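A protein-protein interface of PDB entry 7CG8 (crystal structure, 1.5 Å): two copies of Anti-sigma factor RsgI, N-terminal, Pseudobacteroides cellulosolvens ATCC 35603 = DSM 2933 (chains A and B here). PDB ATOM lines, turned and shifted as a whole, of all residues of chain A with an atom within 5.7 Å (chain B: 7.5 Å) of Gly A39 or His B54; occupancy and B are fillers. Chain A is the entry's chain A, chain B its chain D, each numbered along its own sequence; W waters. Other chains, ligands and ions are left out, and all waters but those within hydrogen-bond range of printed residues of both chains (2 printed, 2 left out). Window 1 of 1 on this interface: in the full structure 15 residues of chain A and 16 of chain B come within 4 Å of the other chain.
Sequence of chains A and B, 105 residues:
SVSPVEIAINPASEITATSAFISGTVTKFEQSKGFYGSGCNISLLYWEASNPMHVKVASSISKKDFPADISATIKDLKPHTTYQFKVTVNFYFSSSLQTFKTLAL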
ATOM      1  N   PHE A  29      31.067   7.478  11.594  1.00  0.00           N
ATOM      2  CA  PHE A  29      30.296   8.655  11.205  1.00  0.00           C
ATOM      3  C   PHE A  29      30.762   9.791  12.119  1.00  0.00           C
ATOM      4  O   PHE A  29      30.245   9.958  13.227  1.00  0.00           O
ATOM      5  CB  PHE A  29      28.794   8.432  11.320  1.00  0.00           C
ATOM      6  CG  PHE A  29      27.984   9.574  10.789  1.00  0.00           C
ATOM      7  CD1 PHE A  29      27.419  10.501  11.651  1.00  0.00           C
ATOM      8  CD2 PHE A  29      27.815   9.749   9.425  1.00  0.00           C
ATOM      9  CE1 PHE A  29      26.680  11.566  11.161  1.00  0.00           C
ATOM     10  CE2 PHE A  29      27.080  10.820   8.926  1.00  0.00           C
ATOM     11  CZ  PHE A  29      26.514  11.725   9.795  1.00  0.00           C
ATOM     12  N   GLN A  31      30.839  13.059  13.804  1.00  0.00           N
ATOM     13  CA  GLN A  31      29.838  14.083  14.055  1.00  0.00           C
ATOM     14  C   GLN A  31      30.518  15.428  14.276  1.00  0.00           C
ATOM     15  O   GLN A  31      31.679  15.504  14.685  1.00  0.00           O
ATOM     16  CB  GLN A  31      28.989  13.726  15.279  1.00  0.00           C
ATOM     17  CG  GLN A  31      28.700  12.237  15.439  1.00  0.00           C
ATOM     18  CD  GLN A  31      27.977  11.922  16.745  1.00  0.00           C
ATOM     19  OE1 GLN A  31      27.219  12.746  17.267  1.00  0.00           O
ATOM     20  NE2 GLN A  31      28.210  10.724  17.277  1.00  0.00           N
ATOM     21  N   PHE A  35      26.575  19.325  16.497  1.00  0.00           N
ATOM     22  CA  PHE A  35      25.575  18.270  16.396  1.00  0.00           C
ATOM     23  C   PHE A  35      26.024  17.010  17.132  1.00  0.00           C
ATOM     24  O   PHE A  35      25.825  15.885  16.658  1.00  0.00           O
ATOM     25  CB  PHE A  35      25.248  17.964  14.936  1.00  0.00           C
ATOM     26  CG  PHE A  35      24.684  19.135  14.179  1.00  0.00           C
ATOM     27  CD1 PHE A  35      23.568  19.812  14.648  1.00  0.00           C
ATOM     28  CD2 PHE A  35      25.268  19.556  12.997  1.00  0.00           C
ATOM     29  CE1 PHE A  35      23.043  20.888  13.951  1.00  0.00           C
ATOM     30  CE2 PHE A  35      24.752  20.633  12.294  1.00  0.00           C
ATOM     31  CZ  PHE A  35      23.637  21.300  12.771  1.00  0.00           C
ATOM     32  N   GLY A  37      25.569  14.187  19.766  1.00  0.00           N
ATOM     33  CA  GLY A  37      24.372  13.575  20.298  1.00  0.00           C
ATOM     34  C   GLY A  37      23.167  13.642  19.389  1.00  0.00           C
ATOM     35  O   GLY A  37      22.071  13.258  19.812  1.00  0.00           O
ATOM     36  N   SER A  38      23.331  14.117  18.157  1.00  0.00           N
ATOM     37  CA  SER A  38      22.213  14.270  17.231  1.00  0.00           C
ATOM     38  C   SER A  38      21.982  12.997  16.418  1.00  0.00           C
ATOM     39  O   SER A  38      20.891  12.420  16.451  1.00  0.00           O
ATOM     40  CB  SER A  38      22.468  15.475  16.320  1.00  0.00           C
ATOM     41  OG  SER A  38      23.497  15.202  15.380  1.00  0.00           O
ATOM     42  N   GLY A  39      22.995  12.547  15.695  1.00  0.00           N
ATOM     43  CA  GLY A  39      22.914  11.299  14.964  1.00  0.00           C
ATOM     44  C   GLY A  39      22.601  11.484  13.493  1.00  0.00           C
ATOM     45  O   GLY A  39      22.657  12.583  12.924  1.00  0.00           O
ATOM     46  N   CYS A  40      22.264  10.357  12.870  1.00  0.00           N
ATOM     47  CA  CYS A  40      21.973  10.305  11.447  1.00  0.00           C
ATOM     48  C   CYS A  40      20.906   9.251  11.204  1.00  0.00           C
ATOM     49  O   CYS A  40      20.609   8.427  12.076  1.00  0.00           O
ATOM     50  CB  CYS A  40      23.231   9.933  10.661  1.00  0.00           C
ATOM     51  SG  CYS A  40      23.874   8.263  10.937  1.00  0.00           S
ATOM     52  N   ASN A  41      20.340   9.276   9.997  1.00  0.00           N
ATOM     53  CA  ASN A  41      19.468   8.207   9.535  1.00  0.00           C
ATOM     54  C   ASN A  41      20.303   7.162   8.807  1.00  0.00           C
ATOM     55  O   ASN A  41      21.155   7.498   7.981  1.00  0.00           O
ATOM     56  CB  ASN A  41      18.387   8.737   8.594  1.00  0.00           C
ATOM     57  CG  ASN A  41      17.534   7.623   8.009  1.00  0.00           C
ATOM     58  OD1 ASN A  41      17.832   7.108   6.942  1.00  0.00           O
ATOM     59  ND2 ASN A  41      16.498   7.215   8.736  1.00  0.00           N
ATOM     60  N   SER A  62      17.368   5.803  13.336  1.00  0.00           N
ATOM     61  CA  SER A  62      18.248   6.869  13.787  1.00  0.00           C
ATOM     62  C   SER A  62      19.307   6.275  14.702  1.00  0.00           C
ATOM     63  O   SER A  62      18.990   5.458  15.568  1.00  0.00           O
ATOM     64  CB  SER A  62      17.449   7.928  14.546  1.00  0.00           C
ATOM     65  OG  SER A  62      16.704   8.750  13.653  1.00  0.00           O
ATOM     66  N   LYS A  63      20.557   6.673  14.504  1.00  0.00           N
ATOM     67  CA  LYS A  63      21.660   6.225  15.342  1.00  0.00           C
ATOM     68  C   LYS A  63      22.587   7.399  15.626  1.00  0.00           C
ATOM     69  O   LYS A  63      22.830   8.243  14.753  1.00  0.00           O
ATOM     70  CB  LYS A  63      22.482   5.116  14.659  1.00  0.00           C
ATOM     71  CG  LYS A  63      21.720   3.830  14.405  1.00  0.00           C
ATOM     72  CD  LYS A  63      21.286   3.158  15.694  1.00  0.00           C
ATOM     73  CE  LYS A  63      22.456   2.584  16.453  1.00  0.00           C
ATOM     74  NZ  LYS A  63      21.999   1.752  17.606  1.00  0.00           N
ATOM     75  N   LYS A  64      23.118   7.459  16.846  1.00  0.00           N
ATOM     76  CA  LYS A  64      24.103   8.487  17.163  1.00  0.00           C
ATOM     77  C   LYS A  64      25.408   7.906  17.689  1.00  0.00           C
ATOM     78  O   LYS A  64      26.326   8.668  18.012  1.00  0.00           O
ATOM     79  CB  LYS A  64      23.578   9.493  18.198  1.00  0.00           C
ATOM     80  CG  LYS A  64      23.240   8.868  19.527  1.00  0.00           C
ATOM     81  CD  LYS A  64      22.676   9.881  20.517  1.00  0.00           C
ATOM     82  CE  LYS A  64      23.017   9.418  21.935  1.00  0.00           C
ATOM     83  NZ  LYS A  64      22.152   9.938  23.020  1.00  0.00           N
ATOM     84  N   PHE A  66      28.475   4.877  17.035  1.00  0.00           N
ATOM     85  CA  PHE A  66      29.066   4.109  15.954  1.00  0.00           C
ATOM     86  C   PHE A  66      30.258   3.318  16.468  1.00  0.00           C
ATOM     87  O   PHE A  66      30.921   3.739  17.426  1.00  0.00           O
ATOM     88  CB  PHE A  66      29.476   5.066  14.819  1.00  0.00           C
ATOM     89  CG  PHE A  66      28.329   5.899  14.336  1.00  0.00           C
ATOM     90  CD1 PHE A  66      27.434   5.408  13.385  1.00  0.00           C
ATOM     91  CD2 PHE A  66      28.077   7.149  14.894  1.00  0.00           C
ATOM     92  CE1 PHE A  66      26.340   6.146  13.003  1.00  0.00           C
ATOM     93  CE2 PHE A  66      26.988   7.893  14.496  1.00  0.00           C
ATOM     94  CZ  PHE A  66      26.111   7.383  13.550  1.00  0.00           C
ATOM     95  N   ASN A  90      21.673   9.219   5.772  1.00  0.00           N
ATOM     96  CA  ASN A  90      21.009  10.485   5.464  1.00  0.00           C
ATOM     97  C   ASN A  90      20.555  10.546   4.004  1.00  0.00           C
ATOM     98  O   ASN A  90      20.498  11.625   3.407  1.00  0.00           O
ATOM     99  CB  ASN A  90      21.898  11.681   5.841  1.00  0.00           C
ATOM    100  CG  ASN A  90      22.271  11.692   7.322  1.00  0.00           C
ATOM    101  OD1 ASN A  90      21.512  11.204   8.153  1.00  0.00           O
ATOM    102  ND2 ASN A  90      23.446  12.227   7.653  1.00  0.00           N
ATOM    103  N   TYR B  46      10.922  14.140   7.618  1.00  0.00           N
ATOM    104  CA  TYR B  46      10.925  15.342   8.445  1.00  0.00           C
ATOM    105  C   TYR B  46      12.223  15.457   9.225  1.00  0.00           C
ATOM    106  O   TYR B  46      12.951  14.481   9.406  1.00  0.00           O
ATOM    107  CB  TYR B  46       9.715  15.390   9.387  1.00  0.00           C
ATOM    108  CG  TYR B  46       9.693  14.337  10.484  1.00  0.00           C
ATOM    109  CD1 TYR B  46       9.303  13.038  10.211  1.00  0.00           C
ATOM    110  CD2 TYR B  46      10.029  14.659  11.791  1.00  0.00           C
ATOM    111  CE1 TYR B  46       9.261  12.077  11.204  1.00  0.00           C
ATOM    112  CE2 TYR B  46       9.988  13.716  12.789  1.00  0.00           C
ATOM    113  CZ  TYR B  46       9.620  12.427  12.496  1.00  0.00           C
ATOM    114  OH  TYR B  46       9.563  11.466  13.484  1.00  0.00           O
ATOM    115  N   TRP B  47      12.503  16.674   9.688  1.00  0.00           N
ATOM    116  CA  TRP B  47      13.748  16.949  10.402  1.00  0.00           C
ATOM    117  C   TRP B  47      13.558  18.222  11.220  1.00  0.00           C
ATOM    118  O   TRP B  47      12.712  19.067  10.902  1.00  0.00           O
ATOM    119  CB  TRP B  47      14.954  17.079   9.442  1.00  0.00           C
ATOM    120  CG  TRP B  47      14.707  18.077   8.352  1.00  0.00           C
ATOM    121  CD1 TRP B  47      15.055  19.396   8.356  1.00  0.00           C
ATOM    122  CD2 TRP B  47      14.044  17.838   7.100  1.00  0.00           C
ATOM    123  NE1 TRP B  47      14.633  19.999   7.190  1.00  0.00           N
ATOM    124  CE2 TRP B  47      14.007  19.062   6.408  1.00  0.00           C
ATOM    125  CE3 TRP B  47      13.462  16.712   6.509  1.00  0.00           C
ATOM    126  CZ2 TRP B  47      13.402  19.197   5.173  1.00  0.00           C
ATOM    127  CZ3 TRP B  47      12.861  16.853   5.276  1.00  0.00           C
ATOM    128  CH2 TRP B  47      12.844  18.082   4.620  1.00  0.00           C
ATOM    129  N   GLU B  48      14.357  18.346  12.288  1.00  0.00           N
ATOM    130  CA  GLU B  48      14.478  19.620  12.980  1.00  0.00           C
ATOM    131  C   GLU B  48      15.124  20.619  12.025  1.00  0.00           C
ATOM    132  O   GLU B  48      16.143  20.313  11.400  1.00  0.00           O
ATOM    133  CB  GLU B  48      15.349  19.464  14.230  1.00  0.00           C
ATOM    134  CG  GLU B  48      14.751  18.516  15.238  1.00  0.00           C
ATOM    135  CD  GLU B  48      15.627  18.300  16.458  1.00  0.00           C
ATOM    136  OE1 GLU B  48      16.509  19.134  16.729  1.00  0.00           O
ATOM    137  OE2 GLU B  48      15.438  17.265  17.119  1.00  0.00           O
ATOM    138  N   ASN B  51      18.765  21.075  12.143  1.00  0.00           N
ATOM    139  CA  ASN B  51      19.622  19.939  11.805  1.00  0.00           C
ATOM    140  C   ASN B  51      19.046  19.182  10.619  1.00  0.00           C
ATOM    141  O   ASN B  51      18.539  18.058  10.752  1.00  0.00           O
ATOM    142  CB  ASN B  51      19.818  19.011  13.002  1.00  0.00           C
ATOM    143  CG  ASN B  51      20.889  17.969  12.746  1.00  0.00           C
ATOM    144  OD1 ASN B  51      21.581  18.021  11.732  1.00  0.00           O
ATOM    145  ND2 ASN B  51      21.006  17.001  13.642  1.00  0.00           N
ATOM    146  N   PRO B  52      19.158  19.754   9.415  1.00  0.00           N
ATOM    147  CA  PRO B  52      18.622  19.089   8.216  1.00  0.00           C
ATOM    148  C   PRO B  52      19.410  17.861   7.795  1.00  0.00           C
ATOM    149  O   PRO B  52      19.003  17.187   6.843  1.00  0.00           O
ATOM    150  CB  PRO B  52      18.696  20.194   7.145  1.00  0.00           C
ATOM    151  CG  PRO B  52      19.862  21.027   7.578  1.00  0.00           C
ATOM    152  CD  PRO B  52      19.806  21.039   9.098  1.00  0.00           C
ATOM    153  N   MET B  53      20.506  17.547   8.481  1.00  0.00           N
ATOM    154  CA  MET B  53      21.325  16.382   8.189  1.00  0.00           C
ATOM    155  C   MET B  53      20.905  15.162   8.994  1.00  0.00           C
ATOM    156  O   MET B  53      21.590  14.136   8.952  1.00  0.00           O
ATOM    157  CB  MET B  53      22.794  16.690   8.492  1.00  0.00           C
ATOM    158  CG  MET B  53      23.437  17.736   7.577  1.00  0.00           C
ATOM    159  SD  MET B  53      23.305  17.392   5.815  1.00  0.00           S
ATOM    160  CE  MET B  53      23.699  15.649   5.741  1.00  0.00           C
ATOM    161  N   HIS B  54      19.831  15.253   9.762  1.00  0.00           N
ATOM    162  CA  HIS B  54      19.295  14.089  10.474  1.00  0.00           C
ATOM    163  C   HIS B  54      17.807  13.991  10.155  1.00  0.00           C
ATOM    164  O   HIS B  54      16.967  14.584  10.836  1.00  0.00           O
ATOM    165  CB  HIS B  54      19.547  14.167  11.970  1.00  0.00           C
ATOM    166  CG  HIS B  54      19.095  12.953  12.722  1.00  0.00           C
ATOM    167  ND1 HIS B  54      19.291  12.800  14.078  1.00  0.00           N
ATOM    168  CD2 HIS B  54      18.444  11.840  12.308  1.00  0.00           C
ATOM    169  CE1 HIS B  54      18.777  11.645  14.468  1.00  0.00           C
ATOM    170  NE2 HIS B  54      18.255  11.046  13.413  1.00  0.00           N
ATOM    171  N   VAL B  55      17.482  13.211   9.140  1.00  0.00           N
ATOM    172  CA  VAL B  55      16.106  13.055   8.688  1.00  0.00           C
ATOM    173  C   VAL B  55      15.459  11.876   9.397  1.00  0.00           C
ATOM    174  O   VAL B  55      16.116  10.920   9.807  1.00  0.00           O
ATOM    175  CB  VAL B  55      16.091  12.878   7.154  1.00  0.00           C
ATOM    176  CG1 VAL B  55      14.705  12.614   6.637  1.00  0.00           C
ATOM    177  CG2 VAL B  55      16.696  14.111   6.492  1.00  0.00           C
ATOM    178  N   LYS B  56      14.144  11.949   9.539  1.00  0.00           N
ATOM    179  CA  LYS B  56      13.334  10.845  10.022  1.00  0.00           C
ATOM    180  C   LYS B  56      12.266  10.533   8.980  1.00  0.00           C
ATOM    181  O   LYS B  56      11.775  11.433   8.284  1.00  0.00           O
ATOM    182  CB  LYS B  56      12.690  11.188  11.358  1.00  0.00           C
ATOM    183  CG  LYS B  56      13.710  11.390  12.493  1.00  0.00           C
ATOM    184  CD  LYS B  56      13.039  11.296  13.861  1.00  0.00           C
ATOM    185  CE  LYS B  56      14.065  11.315  14.997  1.00  0.00           C
ATOM    186  NZ  LYS B  56      14.750   9.998  15.171  1.00  0.00           N
HETATM  187  O   HOH W   1      15.887   8.554  11.125  1.00  0.00           O
HETATM  188  O   HOH W   2      23.432  13.461  10.401  1.00  0.00           O
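A ring nitrogen (ND1) of His B54 lies within hydrogen-bond range of the backbone carbonyl oxygen (O) of Ser A38 (2.9 Å).
The side-chain hydroxyl of Ser A62 is in hydrogen-bond range of a ring nitrogen (NE2) of His B54.
The side-chain amino group (NZ) of Lys B56 is in hydrogen-bond range of the side-chain hydroxyl (OG) of Ser A62, at 2.8 Å.
ND2 of Asn A90 sits at hydrogen-bond distance from O of Met B53, 3.0 Å away.
The backbone carbonyl oxygen of Phe A35 lies close to the side-chain amide oxygen of Gln A31 (3.5 Å).
O of Phe A35 is in hydrogen-bond range of OG of Ser A38 (2.7 Å).
The backbone NH (N) of Cys A40 lies within hydrogen-bond range of the backbone carbonyl oxygen (O) of Lys A63 (2.9 Å).
N of Asn A90 is in hydrogen-bond range of O of Asn A41 (2.8 Å).
The backbone carbonyl oxygen (O) of Tyr B46 sits at hydrogen-bond distance from the backbone NH (N) of Lys B56 (2.8 Å).
The backbone NH (N) of Met B53 lies close to the side-chain amide oxygen (OD1) of Asn B51.
CD1 of Phe A35 touches CG of Asn B51 (3.8 Å).
Asn B51 touches Ser A38.
O of Gly A39 touches ND1 of His B54, 3.6 Å away.
His B54 touches Cys A40.
N of Asn A41 touches CD2 of His B54 (3.9 Å).
Val B55 touches Asn A41 (O to CB, 3.4 Å).
Ser A38 touches just these residues of chain B: Asn B51 and His B54.
Gly A39 touches one residue of chain B.
Of the printed residues of chain B, Cys A40 touches His B54.
Printed residues of chain A within 4 Å of Asn B51: Phe A35 (3.8 Å) and Ser A38 (3.4 Å).
Pro B52 touches none of the printed residues of chain A.
Of chain A, only Ser A38, Gly A39, Cys A40, Asn A41 and Ser A62 come within 4 Å of His B54.
Of the printed residues of chain A, Val B55 touches Asn A41.
The nearest residue of chain B that does not touch Gly A39 is Met B53 (4.4 Å).
The nearest residue of chain A that does not touch His B54 is Asn A90 (4.3 Å).
Of the 9 printed residues of chain B, 5 touch a printed residue of chain A.
Of the 13 printed residues of chain A, 7 touch a printed residue of chain B.
No position is printed for both chains.
Of the 10 pairs that touch across the chains among the printed residues, none has its exchanged pair printed and touching as well.
Water W2 lies within hydrogen-bond range of the backbone carbonyl oxygen (O) of Met B53 (2.4 Å), the backbone carbonyl oxygen (O) of Gly A39 (2.8 Å) and the side-chain amide nitrogen (ND2) of Asn A90 (3.0 Å).
Water W1 lies within hydrogen-bond range of OG of Ser A62, O of Val B55 and ND2 of Asn A41.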
